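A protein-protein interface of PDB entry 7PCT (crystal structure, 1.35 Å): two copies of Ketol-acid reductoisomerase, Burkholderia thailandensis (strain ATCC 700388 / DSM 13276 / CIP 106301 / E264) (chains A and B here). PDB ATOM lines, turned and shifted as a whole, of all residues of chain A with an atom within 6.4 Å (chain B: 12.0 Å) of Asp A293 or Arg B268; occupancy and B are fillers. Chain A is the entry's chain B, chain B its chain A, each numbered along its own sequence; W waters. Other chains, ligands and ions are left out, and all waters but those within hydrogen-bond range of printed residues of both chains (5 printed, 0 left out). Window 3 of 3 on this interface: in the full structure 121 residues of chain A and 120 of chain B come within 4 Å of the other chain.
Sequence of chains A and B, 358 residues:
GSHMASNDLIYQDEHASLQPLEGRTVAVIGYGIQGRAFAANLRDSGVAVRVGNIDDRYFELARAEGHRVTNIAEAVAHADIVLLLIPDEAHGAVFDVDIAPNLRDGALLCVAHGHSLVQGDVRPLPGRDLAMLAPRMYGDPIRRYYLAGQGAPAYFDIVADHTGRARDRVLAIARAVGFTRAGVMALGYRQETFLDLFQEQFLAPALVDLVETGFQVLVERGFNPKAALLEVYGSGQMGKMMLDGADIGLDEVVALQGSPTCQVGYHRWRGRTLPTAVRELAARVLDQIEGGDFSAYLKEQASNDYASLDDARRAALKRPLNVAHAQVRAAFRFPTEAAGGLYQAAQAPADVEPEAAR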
ATOM      1  N   GLN A 201       1.075 -17.589 -24.937  1.00  0.00           N
ATOM      2  CA  GLN A 201       0.676 -17.489 -26.368  1.00  0.00           C
ATOM      3  C   GLN A 201       1.897 -17.454 -27.273  1.00  0.00           C
ATOM      4  O   GLN A 201       1.783 -17.941 -28.410  1.00  0.00           O
ATOM      5  CB  GLN A 201      -0.204 -16.267 -26.587  1.00  0.00           C
ATOM      6  CG  GLN A 201      -1.547 -16.433 -25.902  1.00  0.00           C
ATOM      7  CD  GLN A 201      -2.405 -15.196 -25.889  1.00  0.00           C
ATOM      8  OE1 GLN A 201      -2.373 -14.381 -26.805  1.00  0.00           O
ATOM      9  NE2 GLN A 201      -3.205 -15.061 -24.841  1.00  0.00           N
ATOM     10  N   ASP A 287       0.935  -7.594 -29.571  1.00  0.00           N
ATOM     11  CA  ASP A 287      -0.046  -6.630 -30.141  1.00  0.00           C
ATOM     12  C   ASP A 287      -1.464  -7.190 -29.963  1.00  0.00           C
ATOM     13  O   ASP A 287      -2.359  -6.412 -29.601  1.00  0.00           O
ATOM     14  CB  ASP A 287       0.234  -6.347 -31.615  1.00  0.00           C
ATOM     15  CG  ASP A 287       1.497  -5.555 -31.886  1.00  0.00           C
ATOM     16  OD1 ASP A 287       2.057  -4.961 -30.933  1.00  0.00           O
ATOM     17  OD2 ASP A 287       1.889  -5.514 -33.063  1.00  0.00           O
ATOM     18  N   GLN A 288      -1.674  -8.482 -30.230  1.00  0.00           N
ATOM     19  CA  GLN A 288      -3.007  -9.127 -30.084  1.00  0.00           C
ATOM     20  C   GLN A 288      -3.459  -9.036 -28.623  1.00  0.00           C
ATOM     21  O   GLN A 288      -4.661  -8.832 -28.361  1.00  0.00           O
ATOM     22  CB  GLN A 288      -2.965 -10.596 -30.497  1.00  0.00           C
ATOM     23  CG  GLN A 288      -2.848 -10.843 -31.994  1.00  0.00           C
ATOM     24  CD  GLN A 288      -2.811 -12.327 -32.257  1.00  0.00           C
ATOM     25  OE1 GLN A 288      -2.228 -13.092 -31.483  1.00  0.00           O
ATOM     26  NE2 GLN A 288      -3.407 -12.746 -33.363  1.00  0.00           N
ATOM     27  N   ILE A 289      -2.522  -9.200 -27.698  1.00  0.00           N
ATOM     28  CA  ILE A 289      -2.801  -9.201 -26.239  1.00  0.00           C
ATOM     29  C   ILE A 289      -3.115  -7.769 -25.784  1.00  0.00           C
ATOM     30  O   ILE A 289      -4.140  -7.575 -25.109  1.00  0.00           O
ATOM     31  CB  ILE A 289      -1.607  -9.836 -25.508  1.00  0.00           C
ATOM     32  CG1 ILE A 289      -1.556 -11.347 -25.752  1.00  0.00           C
ATOM     33  CG2 ILE A 289      -1.655  -9.508 -24.024  1.00  0.00           C
ATOM     34  CD1 ILE A 289      -0.236 -11.983 -25.392  1.00  0.00           C
ATOM     35  N   GLU A 290      -2.283  -6.791 -26.143  1.00  0.00           N
ATOM     36  CA  GLU A 290      -2.367  -5.425 -25.563  1.00  0.00           C
ATOM     37  C   GLU A 290      -3.602  -4.695 -26.094  1.00  0.00           C
ATOM     38  O   GLU A 290      -4.108  -3.824 -25.369  1.00  0.00           O
ATOM     39  CB  GLU A 290      -1.088  -4.640 -25.844  1.00  0.00           C
ATOM     40  CG  GLU A 290       0.101  -5.143 -25.048  1.00  0.00           C
ATOM     41  CD  GLU A 290       1.373  -4.346 -25.260  1.00  0.00           C
ATOM     42  OE1 GLU A 290       1.487  -3.696 -26.323  1.00  0.00           O
ATOM     43  OE2 GLU A 290       2.256  -4.392 -24.370  1.00  0.00           O
ATOM     44  N   GLY A 291      -4.075  -5.042 -27.296  1.00  0.00           N
ATOM     45  CA  GLY A 291      -5.094  -4.256 -28.018  1.00  0.00           C
ATOM     46  C   GLY A 291      -6.493  -4.851 -27.933  1.00  0.00           C
ATOM     47  O   GLY A 291      -7.407  -4.255 -28.523  1.00  0.00           O
ATOM     48  N   GLY A 292      -6.669  -5.974 -27.231  1.00  0.00           N
ATOM     49  CA  GLY A 292      -7.996  -6.571 -26.977  1.00  0.00           C
ATOM     50  C   GLY A 292      -8.376  -7.682 -27.951  1.00  0.00           C
ATOM     51  O   GLY A 292      -9.425  -8.299 -27.732  1.00  0.00           O
ATOM     52  N   ASP A 293      -7.578  -7.928 -28.993  1.00  0.00           N
ATOM     53  CA  ASP A 293      -7.862  -8.981 -30.007  1.00  0.00           C
ATOM     54  C   ASP A 293      -7.937 -10.337 -29.294  1.00  0.00           C
ATOM     55  O   ASP A 293      -8.925 -11.083 -29.493  1.00  0.00           O
ATOM     56  CB  ASP A 293      -6.829  -8.937 -31.138  1.00  0.00           C
ATOM     57  CG  ASP A 293      -6.974 -10.029 -32.189  1.00  0.00           C
ATOM     58  OD1 ASP A 293      -6.870 -11.204 -31.825  1.00  0.00           O
ATOM     59  OD2 ASP A 293      -7.166  -9.694 -33.374  1.00  0.00           O
ATOM     60  N   PHE A 294      -6.950 -10.677 -28.468  1.00  0.00           N
ATOM     61  CA  PHE A 294      -7.002 -11.970 -27.745  1.00  0.00           C
ATOM     62  C   PHE A 294      -8.253 -12.036 -26.860  1.00  0.00           C
ATOM     63  O   PHE A 294      -8.899 -13.099 -26.829  1.00  0.00           O
ATOM     64  CB  PHE A 294      -5.753 -12.247 -26.915  1.00  0.00           C
ATOM     65  CG  PHE A 294      -5.946 -13.491 -26.093  1.00  0.00           C
ATOM     66  CD1 PHE A 294      -5.967 -14.739 -26.698  1.00  0.00           C
ATOM     67  CD2 PHE A 294      -6.219 -13.405 -24.739  1.00  0.00           C
ATOM     68  CE1 PHE A 294      -6.199 -15.884 -25.951  1.00  0.00           C
ATOM     69  CE2 PHE A 294      -6.445 -14.547 -23.995  1.00  0.00           C
ATOM     70  CZ  PHE A 294      -6.437 -15.784 -24.600  1.00  0.00           C
ATOM     71  N   SER A 295      -8.579 -10.964 -26.132  1.00  0.00           N
ATOM     72  CA  SER A 295      -9.726 -10.961 -25.188  1.00  0.00           C
ATOM     73  C   SER A 295     -11.024 -11.282 -25.946  1.00  0.00           C
ATOM     74  O   SER A 295     -11.845 -12.064 -25.423  1.00  0.00           O
ATOM     75  CB  SER A 295      -9.817  -9.659 -24.421  1.00  0.00           C
ATOM     76  OG  SER A 295      -8.645  -9.455 -23.645  1.00  0.00           O
ATOM     77  N   ALA A 296     -11.198 -10.724 -27.144  1.00  0.00           N
ATOM     78  CA  ALA A 296     -12.366 -10.995 -28.017  1.00  0.00           C
ATOM     79  C   ALA A 296     -12.347 -12.456 -28.482  1.00  0.00           C
ATOM     80  O   ALA A 296     -13.414 -13.107 -28.467  1.00  0.00           O
ATOM     81  CB  ALA A 296     -12.380 -10.038 -29.182  1.00  0.00           C
ATOM     82  N   TYR A 297     -11.166 -12.975 -28.826  1.00  0.00           N
ATOM     83  CA  TYR A 297     -10.984 -14.383 -29.270  1.00  0.00           C
ATOM     84  C   TYR A 297     -11.366 -15.312 -28.114  1.00  0.00           C
ATOM     85  O   TYR A 297     -12.118 -16.280 -28.349  1.00  0.00           O
ATOM     86  CB  TYR A 297      -9.554 -14.593 -29.764  1.00  0.00           C
ATOM     87  CG  TYR A 297      -9.168 -15.996 -30.156  1.00  0.00           C
ATOM     88  CD1 TYR A 297      -9.392 -16.480 -31.435  1.00  0.00           C
ATOM     89  CD2 TYR A 297      -8.521 -16.824 -29.254  1.00  0.00           C
ATOM     90  CE1 TYR A 297      -8.989 -17.754 -31.802  1.00  0.00           C
ATOM     91  CE2 TYR A 297      -8.123 -18.106 -29.599  1.00  0.00           C
ATOM     92  CZ  TYR A 297      -8.353 -18.569 -30.881  1.00  0.00           C
ATOM     93  OH  TYR A 297      -7.968 -19.828 -31.236  1.00  0.00           O
ATOM     94  N   LEU A 298     -10.868 -15.024 -26.907  1.00  0.00           N
ATOM     95  CA  LEU A 298     -11.168 -15.809 -25.680  1.00  0.00           C
ATOM     96  C   LEU A 298     -12.677 -15.837 -25.432  1.00  0.00           C
ATOM     97  O   LEU A 298     -13.205 -16.920 -25.131  1.00  0.00           O
ATOM     98  CB  LEU A 298     -10.457 -15.192 -24.473  1.00  0.00           C
ATOM     99  CG  LEU A 298     -10.729 -15.882 -23.139  1.00  0.00           C
ATOM    100  CD1 LEU A 298     -10.333 -17.353 -23.195  1.00  0.00           C
ATOM    101  CD2 LEU A 298     -10.024 -15.159 -21.998  1.00  0.00           C
ATOM    102  N   ARG B 221       9.433  -3.806 -24.932  1.00  0.00           N
ATOM    103  CA  ARG B 221       8.009  -3.398 -24.927  1.00  0.00           C
ATOM    104  C   ARG B 221       7.615  -2.863 -23.544  1.00  0.00           C
ATOM    105  O   ARG B 221       6.411  -2.683 -23.318  1.00  0.00           O
ATOM    106  CB  ARG B 221       7.165  -4.580 -25.403  1.00  0.00           C
ATOM    107  CG  ARG B 221       7.316  -4.822 -26.897  1.00  0.00           C
ATOM    108  CD  ARG B 221       6.597  -3.775 -27.720  1.00  0.00           C
ATOM    109  NE  ARG B 221       5.144  -3.919 -27.674  1.00  0.00           N
ATOM    110  CZ  ARG B 221       4.409  -4.566 -28.576  1.00  0.00           C
ATOM    111  NH1 ARG B 221       4.976  -5.124 -29.632  1.00  0.00           N
ATOM    112  NH2 ARG B 221       3.099  -4.644 -28.420  1.00  0.00           N
ATOM    113  N   ASP B 251       1.675 -31.230 -24.777  1.00  0.00           N
ATOM    114  CA  ASP B 251       0.303 -30.720 -25.012  1.00  0.00           C
ATOM    115  C   ASP B 251      -0.589 -31.138 -23.838  1.00  0.00           C
ATOM    116  O   ASP B 251      -1.492 -30.348 -23.426  1.00  0.00           O
ATOM    117  CB  ASP B 251      -0.188 -31.185 -26.377  1.00  0.00           C
ATOM    118  CG  ASP B 251       0.581 -30.541 -27.523  1.00  0.00           C
ATOM    119  OD1 ASP B 251       0.733 -29.312 -27.506  1.00  0.00           O
ATOM    120  OD2 ASP B 251       1.043 -31.270 -28.401  1.00  0.00           O
ATOM    121  N   VAL B 254      -0.352 -28.832 -20.739  1.00  0.00           N
ATOM    122  CA  VAL B 254      -1.209 -27.625 -20.921  1.00  0.00           C
ATOM    123  C   VAL B 254      -2.671 -27.999 -20.652  1.00  0.00           C
ATOM    124  O   VAL B 254      -3.340 -27.243 -19.961  1.00  0.00           O
ATOM    125  CB  VAL B 254      -1.011 -26.972 -22.298  1.00  0.00           C
ATOM    126  CG1 VAL B 254      -2.021 -25.855 -22.542  1.00  0.00           C
ATOM    127  CG2 VAL B 254       0.419 -26.468 -22.454  1.00  0.00           C
ATOM    128  N   ALA B 255      -3.148 -29.126 -21.166  1.00  0.00           N
ATOM    129  CA  ALA B 255      -4.551 -29.564 -20.955  1.00  0.00           C
ATOM    130  C   ALA B 255      -4.844 -29.787 -19.477  1.00  0.00           C
ATOM    131  O   ALA B 255      -5.986 -29.533 -19.055  1.00  0.00           O
ATOM    132  CB  ALA B 255      -4.846 -30.806 -21.742  1.00  0.00           C
ATOM    133  N   SER B 259      -5.051 -22.976 -17.038  1.00  0.00           N
ATOM    134  CA  SER B 259      -6.411 -22.389 -16.962  1.00  0.00           C
ATOM    135  C   SER B 259      -7.022 -22.471 -18.360  1.00  0.00           C
ATOM    136  O   SER B 259      -6.303 -22.547 -19.356  1.00  0.00           O
ATOM    137  CB  SER B 259      -6.369 -20.966 -16.472  1.00  0.00           C
ATOM    138  OG  SER B 259      -5.843 -20.108 -17.484  1.00  0.00           O
ATOM    139  N   PRO B 260      -8.352 -22.374 -18.541  1.00  0.00           N
ATOM    140  CA  PRO B 260      -8.923 -22.289 -19.883  1.00  0.00           C
ATOM    141  C   PRO B 260      -8.361 -21.108 -20.684  1.00  0.00           C
ATOM    142  O   PRO B 260      -8.143 -21.241 -21.892  1.00  0.00           O
ATOM    143  CB  PRO B 260     -10.432 -22.170 -19.611  1.00  0.00           C
ATOM    144  CG  PRO B 260     -10.592 -22.903 -18.287  1.00  0.00           C
ATOM    145  CD  PRO B 260      -9.378 -22.456 -17.496  1.00  0.00           C
ATOM    146  N   THR B 261      -8.099 -19.985 -20.015  1.00  0.00           N
ATOM    147  CA  THR B 261      -7.473 -18.797 -20.642  1.00  0.00           C
ATOM    148  C   THR B 261      -6.128 -19.200 -21.249  1.00  0.00           C
ATOM    149  O   THR B 261      -5.860 -18.869 -22.409  1.00  0.00           O
ATOM    150  CB  THR B 261      -7.256 -17.681 -19.623  1.00  0.00           C
ATOM    151  OG1 THR B 261      -8.514 -17.458 -18.982  1.00  0.00           O
ATOM    152  CG2 THR B 261      -6.734 -16.416 -20.263  1.00  0.00           C
ATOM    153  N   CYS B 262      -5.310 -19.890 -20.468  1.00  0.00           N
ATOM    154  CA  CYS B 262      -3.982 -20.365 -20.905  1.00  0.00           C
ATOM    155  C   CYS B 262      -4.140 -21.338 -22.076  1.00  0.00           C
ATOM    156  O   CYS B 262      -3.429 -21.186 -23.072  1.00  0.00           O
ATOM    157  CB  CYS B 262      -3.293 -21.057 -19.743  1.00  0.00           C
ATOM    158  SG  CYS B 262      -1.787 -21.923 -20.229  1.00  0.00           S
ATOM    159  N   GLN B 263      -5.040 -22.314 -21.979  1.00  0.00           N
ATOM    160  CA  GLN B 263      -5.187 -23.348 -23.033  1.00  0.00           C
ATOM    161  C   GLN B 263      -5.660 -22.702 -24.340  1.00  0.00           C
ATOM    162  O   GLN B 263      -5.169 -23.082 -25.423  1.00  0.00           O
ATOM    163  CB  GLN B 263      -6.165 -24.424 -22.581  1.00  0.00           C
ATOM    164  CG  GLN B 263      -5.684 -25.192 -21.368  1.00  0.00           C
ATOM    165  CD  GLN B 263      -6.505 -26.431 -21.111  1.00  0.00           C
ATOM    166  OE1 GLN B 263      -6.843 -27.178 -22.024  1.00  0.00           O
ATOM    167  NE2 GLN B 263      -6.794 -26.708 -19.845  1.00  0.00           N
ATOM    168  N   VAL B 264      -6.615 -21.774 -24.268  1.00  0.00           N
ATOM    169  CA  VAL B 264      -7.127 -21.081 -25.487  1.00  0.00           C
ATOM    170  C   VAL B 264      -5.969 -20.288 -26.117  1.00  0.00           C
ATOM    171  O   VAL B 264      -5.791 -20.344 -27.354  1.00  0.00           O
ATOM    172  CB  VAL B 264      -8.335 -20.187 -25.154  1.00  0.00           C
ATOM    173  CG1 VAL B 264      -8.607 -19.194 -26.272  1.00  0.00           C
ATOM    174  CG2 VAL B 264      -9.576 -21.019 -24.836  1.00  0.00           C
ATOM    175  N   GLY B 265      -5.179 -19.581 -25.308  1.00  0.00           N
ATOM    176  CA  GLY B 265      -4.010 -18.839 -25.812  1.00  0.00           C
ATOM    177  C   GLY B 265      -2.995 -19.756 -26.481  1.00  0.00           C
ATOM    178  O   GLY B 265      -2.552 -19.482 -27.618  1.00  0.00           O
ATOM    179  N   TYR B 266      -2.606 -20.822 -25.800  1.00  0.00           N
ATOM    180  CA  TYR B 266      -1.593 -21.797 -26.275  1.00  0.00           C
ATOM    181  C   TYR B 266      -2.019 -22.361 -27.629  1.00  0.00           C
ATOM    182  O   TYR B 266      -1.236 -22.351 -28.587  1.00  0.00           O
ATOM    183  CB  TYR B 266      -1.449 -22.898 -25.232  1.00  0.00           C
ATOM    184  CG  TYR B 266      -0.530 -24.032 -25.588  1.00  0.00           C
ATOM    185  CD1 TYR B 266      -1.033 -25.210 -26.114  1.00  0.00           C
ATOM    186  CD2 TYR B 266       0.829 -23.956 -25.348  1.00  0.00           C
ATOM    187  CE1 TYR B 266      -0.207 -26.281 -26.404  1.00  0.00           C
ATOM    188  CE2 TYR B 266       1.671 -25.023 -25.620  1.00  0.00           C
ATOM    189  CZ  TYR B 266       1.150 -26.191 -26.147  1.00  0.00           C
ATOM    190  OH  TYR B 266       1.979 -27.245 -26.400  1.00  0.00           O
ATOM    191  N   HIS B 267      -3.263 -22.820 -27.728  1.00  0.00           N
ATOM    192  CA  HIS B 267      -3.761 -23.475 -28.964  1.00  0.00           C
ATOM    193  C   HIS B 267      -4.026 -22.448 -30.068  1.00  0.00           C
ATOM    194  O   HIS B 267      -4.202 -22.880 -31.213  1.00  0.00           O
ATOM    195  CB  HIS B 267      -4.959 -24.369 -28.652  1.00  0.00           C
ATOM    196  CG  HIS B 267      -4.531 -25.673 -28.085  1.00  0.00           C
ATOM    197  ND1 HIS B 267      -3.763 -26.556 -28.820  1.00  0.00           N
ATOM    198  CD2 HIS B 267      -4.689 -26.231 -26.866  1.00  0.00           C
ATOM    199  CE1 HIS B 267      -3.492 -27.618 -28.087  1.00  0.00           C
ATOM    200  NE2 HIS B 267      -4.046 -27.439 -26.885  1.00  0.00           N
ATOM    201  N   ARG B 268      -4.058 -21.147 -29.772  1.00  0.00           N
ATOM    202  CA  ARG B 268      -4.168 -20.131 -30.850  1.00  0.00           C
ATOM    203  C   ARG B 268      -2.874 -20.113 -31.679  1.00  0.00           C
ATOM    204  O   ARG B 268      -2.953 -19.853 -32.892  1.00  0.00           O
ATOM    205  CB  ARG B 268      -4.441 -18.738 -30.282  1.00  0.00           C
ATOM    206  CG  ARG B 268      -4.823 -17.741 -31.367  1.00  0.00           C
ATOM    207  CD  ARG B 268      -5.143 -16.362 -30.830  1.00  0.00           C
ATOM    208  NE  ARG B 268      -5.906 -15.627 -31.824  1.00  0.00           N
ATOM    209  CZ  ARG B 268      -6.237 -14.344 -31.743  1.00  0.00           C
ATOM    210  NH1 ARG B 268      -5.831 -13.614 -30.718  1.00  0.00           N
ATOM    211  NH2 ARG B 268      -6.955 -13.793 -32.706  1.00  0.00           N
ATOM    212  N   TRP B 269      -1.728 -20.405 -31.055  1.00  0.00           N
ATOM    213  CA  TRP B 269      -0.396 -20.260 -31.693  1.00  0.00           C
ATOM    214  C   TRP B 269       0.369 -21.578 -31.805  1.00  0.00           C
ATOM    215  O   TRP B 269       1.320 -21.590 -32.569  1.00  0.00           O
ATOM    216  CB  TRP B 269       0.398 -19.184 -30.955  1.00  0.00           C
ATOM    217  CG  TRP B 269      -0.044 -17.832 -31.416  1.00  0.00           C
ATOM    218  CD1 TRP B 269      -0.857 -16.955 -30.761  1.00  0.00           C
ATOM    219  CD2 TRP B 269       0.211 -17.258 -32.707  1.00  0.00           C
ATOM    220  NE1 TRP B 269      -1.082 -15.852 -31.536  1.00  0.00           N
ATOM    221  CE2 TRP B 269      -0.448 -16.011 -32.739  1.00  0.00           C
ATOM    222  CE3 TRP B 269       0.954 -17.659 -33.824  1.00  0.00           C
ATOM    223  CZ2 TRP B 269      -0.376 -15.161 -33.842  1.00  0.00           C
ATOM    224  CZ3 TRP B 269       1.012 -16.826 -34.919  1.00  0.00           C
ATOM    225  CH2 TRP B 269       0.359 -15.592 -34.923  1.00  0.00           C
ATOM    226  N   ARG B 270      -0.050 -22.649 -31.125  1.00  0.00           N
ATOM    227  CA  ARG B 270       0.599 -23.979 -31.218  1.00  0.00           C
ATOM    228  C   ARG B 270       0.675 -24.393 -32.695  1.00  0.00           C
ATOM    229  O   ARG B 270      -0.351 -24.325 -33.401  1.00  0.00           O
ATOM    230  CB  ARG B 270      -0.164 -24.997 -30.370  1.00  0.00           C
ATOM    231  CG  ARG B 270       0.405 -26.404 -30.430  1.00  0.00           C
ATOM    232  CD  ARG B 270       1.749 -26.586 -29.746  1.00  0.00           C
ATOM    233  NE  ARG B 270       2.007 -28.016 -29.703  1.00  0.00           N
ATOM    234  CZ  ARG B 270       2.688 -28.709 -30.608  1.00  0.00           C
ATOM    235  NH1 ARG B 270       3.323 -28.097 -31.595  1.00  0.00           N
ATOM    236  NH2 ARG B 270       2.769 -30.024 -30.491  1.00  0.00           N
ATOM    237  N   GLY B 271       1.865 -24.788 -33.150  1.00  0.00           N
ATOM    238  CA  GLY B 271       2.103 -25.240 -34.532  1.00  0.00           C
ATOM    239  C   GLY B 271       2.260 -24.089 -35.507  1.00  0.00           C
ATOM    240  O   GLY B 271       2.413 -24.379 -36.710  1.00  0.00           O
ATOM    241  N   ARG B 272       2.256 -22.835 -35.042  1.00  0.00           N
ATOM    242  CA  ARG B 272       2.224 -21.645 -35.946  1.00  0.00           C
ATOM    243  C   ARG B 272       3.319 -20.623 -35.610  1.00  0.00           C
ATOM    244  O   ARG B 272       3.370 -19.600 -36.304  1.00  0.00           O
ATOM    245  CB  ARG B 272       0.853 -20.959 -35.893  1.00  0.00           C
ATOM    246  CG  ARG B 272      -0.308 -21.879 -36.241  1.00  0.00           C
ATOM    247  CD  ARG B 272      -1.575 -21.147 -36.641  1.00  0.00           C
ATOM    248  NE  ARG B 272      -1.936 -20.092 -35.703  1.00  0.00           N
ATOM    249  CZ  ARG B 272      -1.939 -18.780 -35.957  1.00  0.00           C
ATOM    250  NH1 ARG B 272      -2.291 -17.932 -35.001  1.00  0.00           N
ATOM    251  NH2 ARG B 272      -1.605 -18.311 -37.149  1.00  0.00           N
ATOM    252  N   THR B 273       4.180 -20.860 -34.618  1.00  0.00           N
ATOM    253  CA  THR B 273       5.115 -19.806 -34.132  1.00  0.00           C
ATOM    254  C   THR B 273       6.386 -19.702 -34.983  1.00  0.00           C
ATOM    255  O   THR B 273       7.013 -18.625 -34.936  1.00  0.00           O
ATOM    256  CB  THR B 273       5.498 -20.020 -32.663  1.00  0.00           C
ATOM    257  OG1 THR B 273       6.185 -21.268 -32.547  1.00  0.00           O
ATOM    258  CG2 THR B 273       4.293 -19.952 -31.753  1.00  0.00           C
ATOM    259  N   LEU B 274       6.804 -20.764 -35.674  1.00  0.00           N
ATOM    260  CA  LEU B 274       8.168 -20.805 -36.269  1.00  0.00           C
ATOM    261  C   LEU B 274       8.129 -20.654 -37.784  1.00  0.00           C
ATOM    262  O   LEU B 274       7.349 -21.311 -38.470  1.00  0.00           O
ATOM    263  CB  LEU B 274       8.870 -22.100 -35.864  1.00  0.00           C
ATOM    264  CG  LEU B 274       8.970 -22.326 -34.358  1.00  0.00           C
ATOM    265  CD1 LEU B 274       9.648 -23.650 -34.048  1.00  0.00           C
ATOM    266  CD2 LEU B 274       9.697 -21.172 -33.679  1.00  0.00           C
HETATM  267  O   HOH W   1      -3.426 -17.287 -22.948  1.00  0.00           O
HETATM  268  O   HOH W   2       4.198  -2.739 -25.196  1.00  0.00           O
HETATM  269  O   HOH W   3      -7.262 -21.513 -29.331  1.00  0.00           O
HETATM  270  O   HOH W   4      -3.777 -15.304 -34.888  1.00  0.00           O
HETATM  271  O   HOH W   5      -3.449 -13.925 -29.212  1.00  0.00           O
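The side-chain carboxylate (OD1) of Asp A287 is in salt-bridge range of the guanidinium group (NH2) of Arg B221 (2.7 Å).
NH2 of Arg B221 lies within salt-bridge range of OE1 of Glu A290, at 2.8 Å.
The guanidinium group (NH2) of Arg B268 is in salt-bridge range of the side-chain carboxylate (OD1) of Asp A293 (2.7 Å).
NE1 of Trp B269 sits at hydrogen-bond distance from OE1 of Gln A288.
N of Thr B261 lies close to OG of Ser B259 (3.4 Å).
The backbone carbonyl oxygen (O) of Arg B268 lies within hydrogen-bond range of the guanidinium group (NH1) of Arg B272, 2.9 Å away.
The backbone carbonyl oxygen of Gln A288 is in hydrogen-bond range of the backbone NH of Asp A293, at 3.1 Å.
The backbone NH of Phe A294 sits at hydrogen-bond distance from the backbone carbonyl oxygen of Gln A288, 2.9 Å away.
CG of Gln A201 touches CA of Gly B265, 3.4 Å away.
Gln A201 touches Trp B269.
NH1 of Arg B268 touches CD of Gln A288 (3.6 Å).
Phe A294 touches Thr B261.
Gly B265 touches Phe A294.
CA of Phe A294 touches NH1 of Arg B268, 3.6 Å away.
CE2 of Tyr A297 touches CG1 of Val B264, at 3.5 Å.
NE of Arg B268 touches CD1 of Tyr A297, at 3.6 Å.
Thr B261 touches Leu A298.
CD1 of Leu A298 touches CG1 of Val B264 (3.98 Å).
Of chain B, only Gly B265 and Trp B269 come within 4 Å of Gln A201.
Printed residues of chain B within 4 Å of Asp A287: Arg B221.
Gln A288 touches two residues of chain B.
No residue of chain B comes within 4 Å of Ile A289.
Gly A291 touches none of the printed residues of chain B.
No residue of chain B comes within 4 Å of Gly A292.
Asp A293 touches just one residue of chain B: Arg B268 (2.7 Å).
Phe A294 touches just these residues of chain B: Thr B261, Gly B265 and Arg B268.
Printed residues of chain B within 4 Å of Tyr A297: Val B264 (3.5 Å) and Arg B268 (3.6 Å).
Cys B262 touches none of the printed residues of chain A.
Of the printed residues of chain A, Val B264 touches Tyr A297 (3.5 Å) and Leu A298 (3.98 Å).
Of the printed residues of chain A, Arg B268 touches Gln A288 (3.6 Å), Asp A293 (2.7 Å), Phe A294 (3.6 Å) and Tyr A297 (3.6 Å).
Leu B274 touches none of the printed residues of chain A.
The nearest residue of chain B that does not touch Asp A293 is Trp B269 (7.4 Å).
The nearest residue of chain A that does not touch Arg B268 is Gln A201 (5.3 Å).
Of the 20 printed residues of chain B, 6 touch a printed residue of chain A.
Hydrophobic or aromatic side chains of chain B that line the printed part of chain A: Val B264 and Trp B269.
Of the 13 printed residues of chain A, 8 touch a printed residue of chain B.
Printed residues of chain A that touch a printed residue of chain B: Gln A201, Asp A287, Gln A288, Glu A290, Asp A293, Phe A294, Tyr A297 and Leu A298.
Among the printed residues, Asp or Glu carboxylates within 4 Å of a Lys or Arg side-chain nitrogen of the other chain: Asp A287 with Arg B221 (2.7 Å), Glu A290 with Arg B221 (2.8 Å) and Asp A293 with Arg B268 (2.7 Å).
No position is printed for both chains.
Water W3 lies within hydrogen-bond range of OH of Tyr A297, O of Val B264 and N of Arg B268.
Water W5 lies within hydrogen-bond range of OE1 of Gln A201 (2.7 Å), OE1 of Gln A288 (2.7 Å) and NH1 of Arg B268 (2.8 Å).
Water W2 lies within hydrogen-bond range of the side-chain carboxylate (OE2) of Glu A290 (2.7 Å) and the backbone carbonyl oxygen (O) of Arg B221 (2.9 Å).
Water W1 bridges the side-chain amide nitrogen of Gln A201 (2.9 Å) and the backbone carbonyl oxygen of Thr B261 (3.0 Å).
Water W4 bridges NE2 of Gln A288 (3.0 Å) and NH1 of Arg B272 (3.0 Å).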
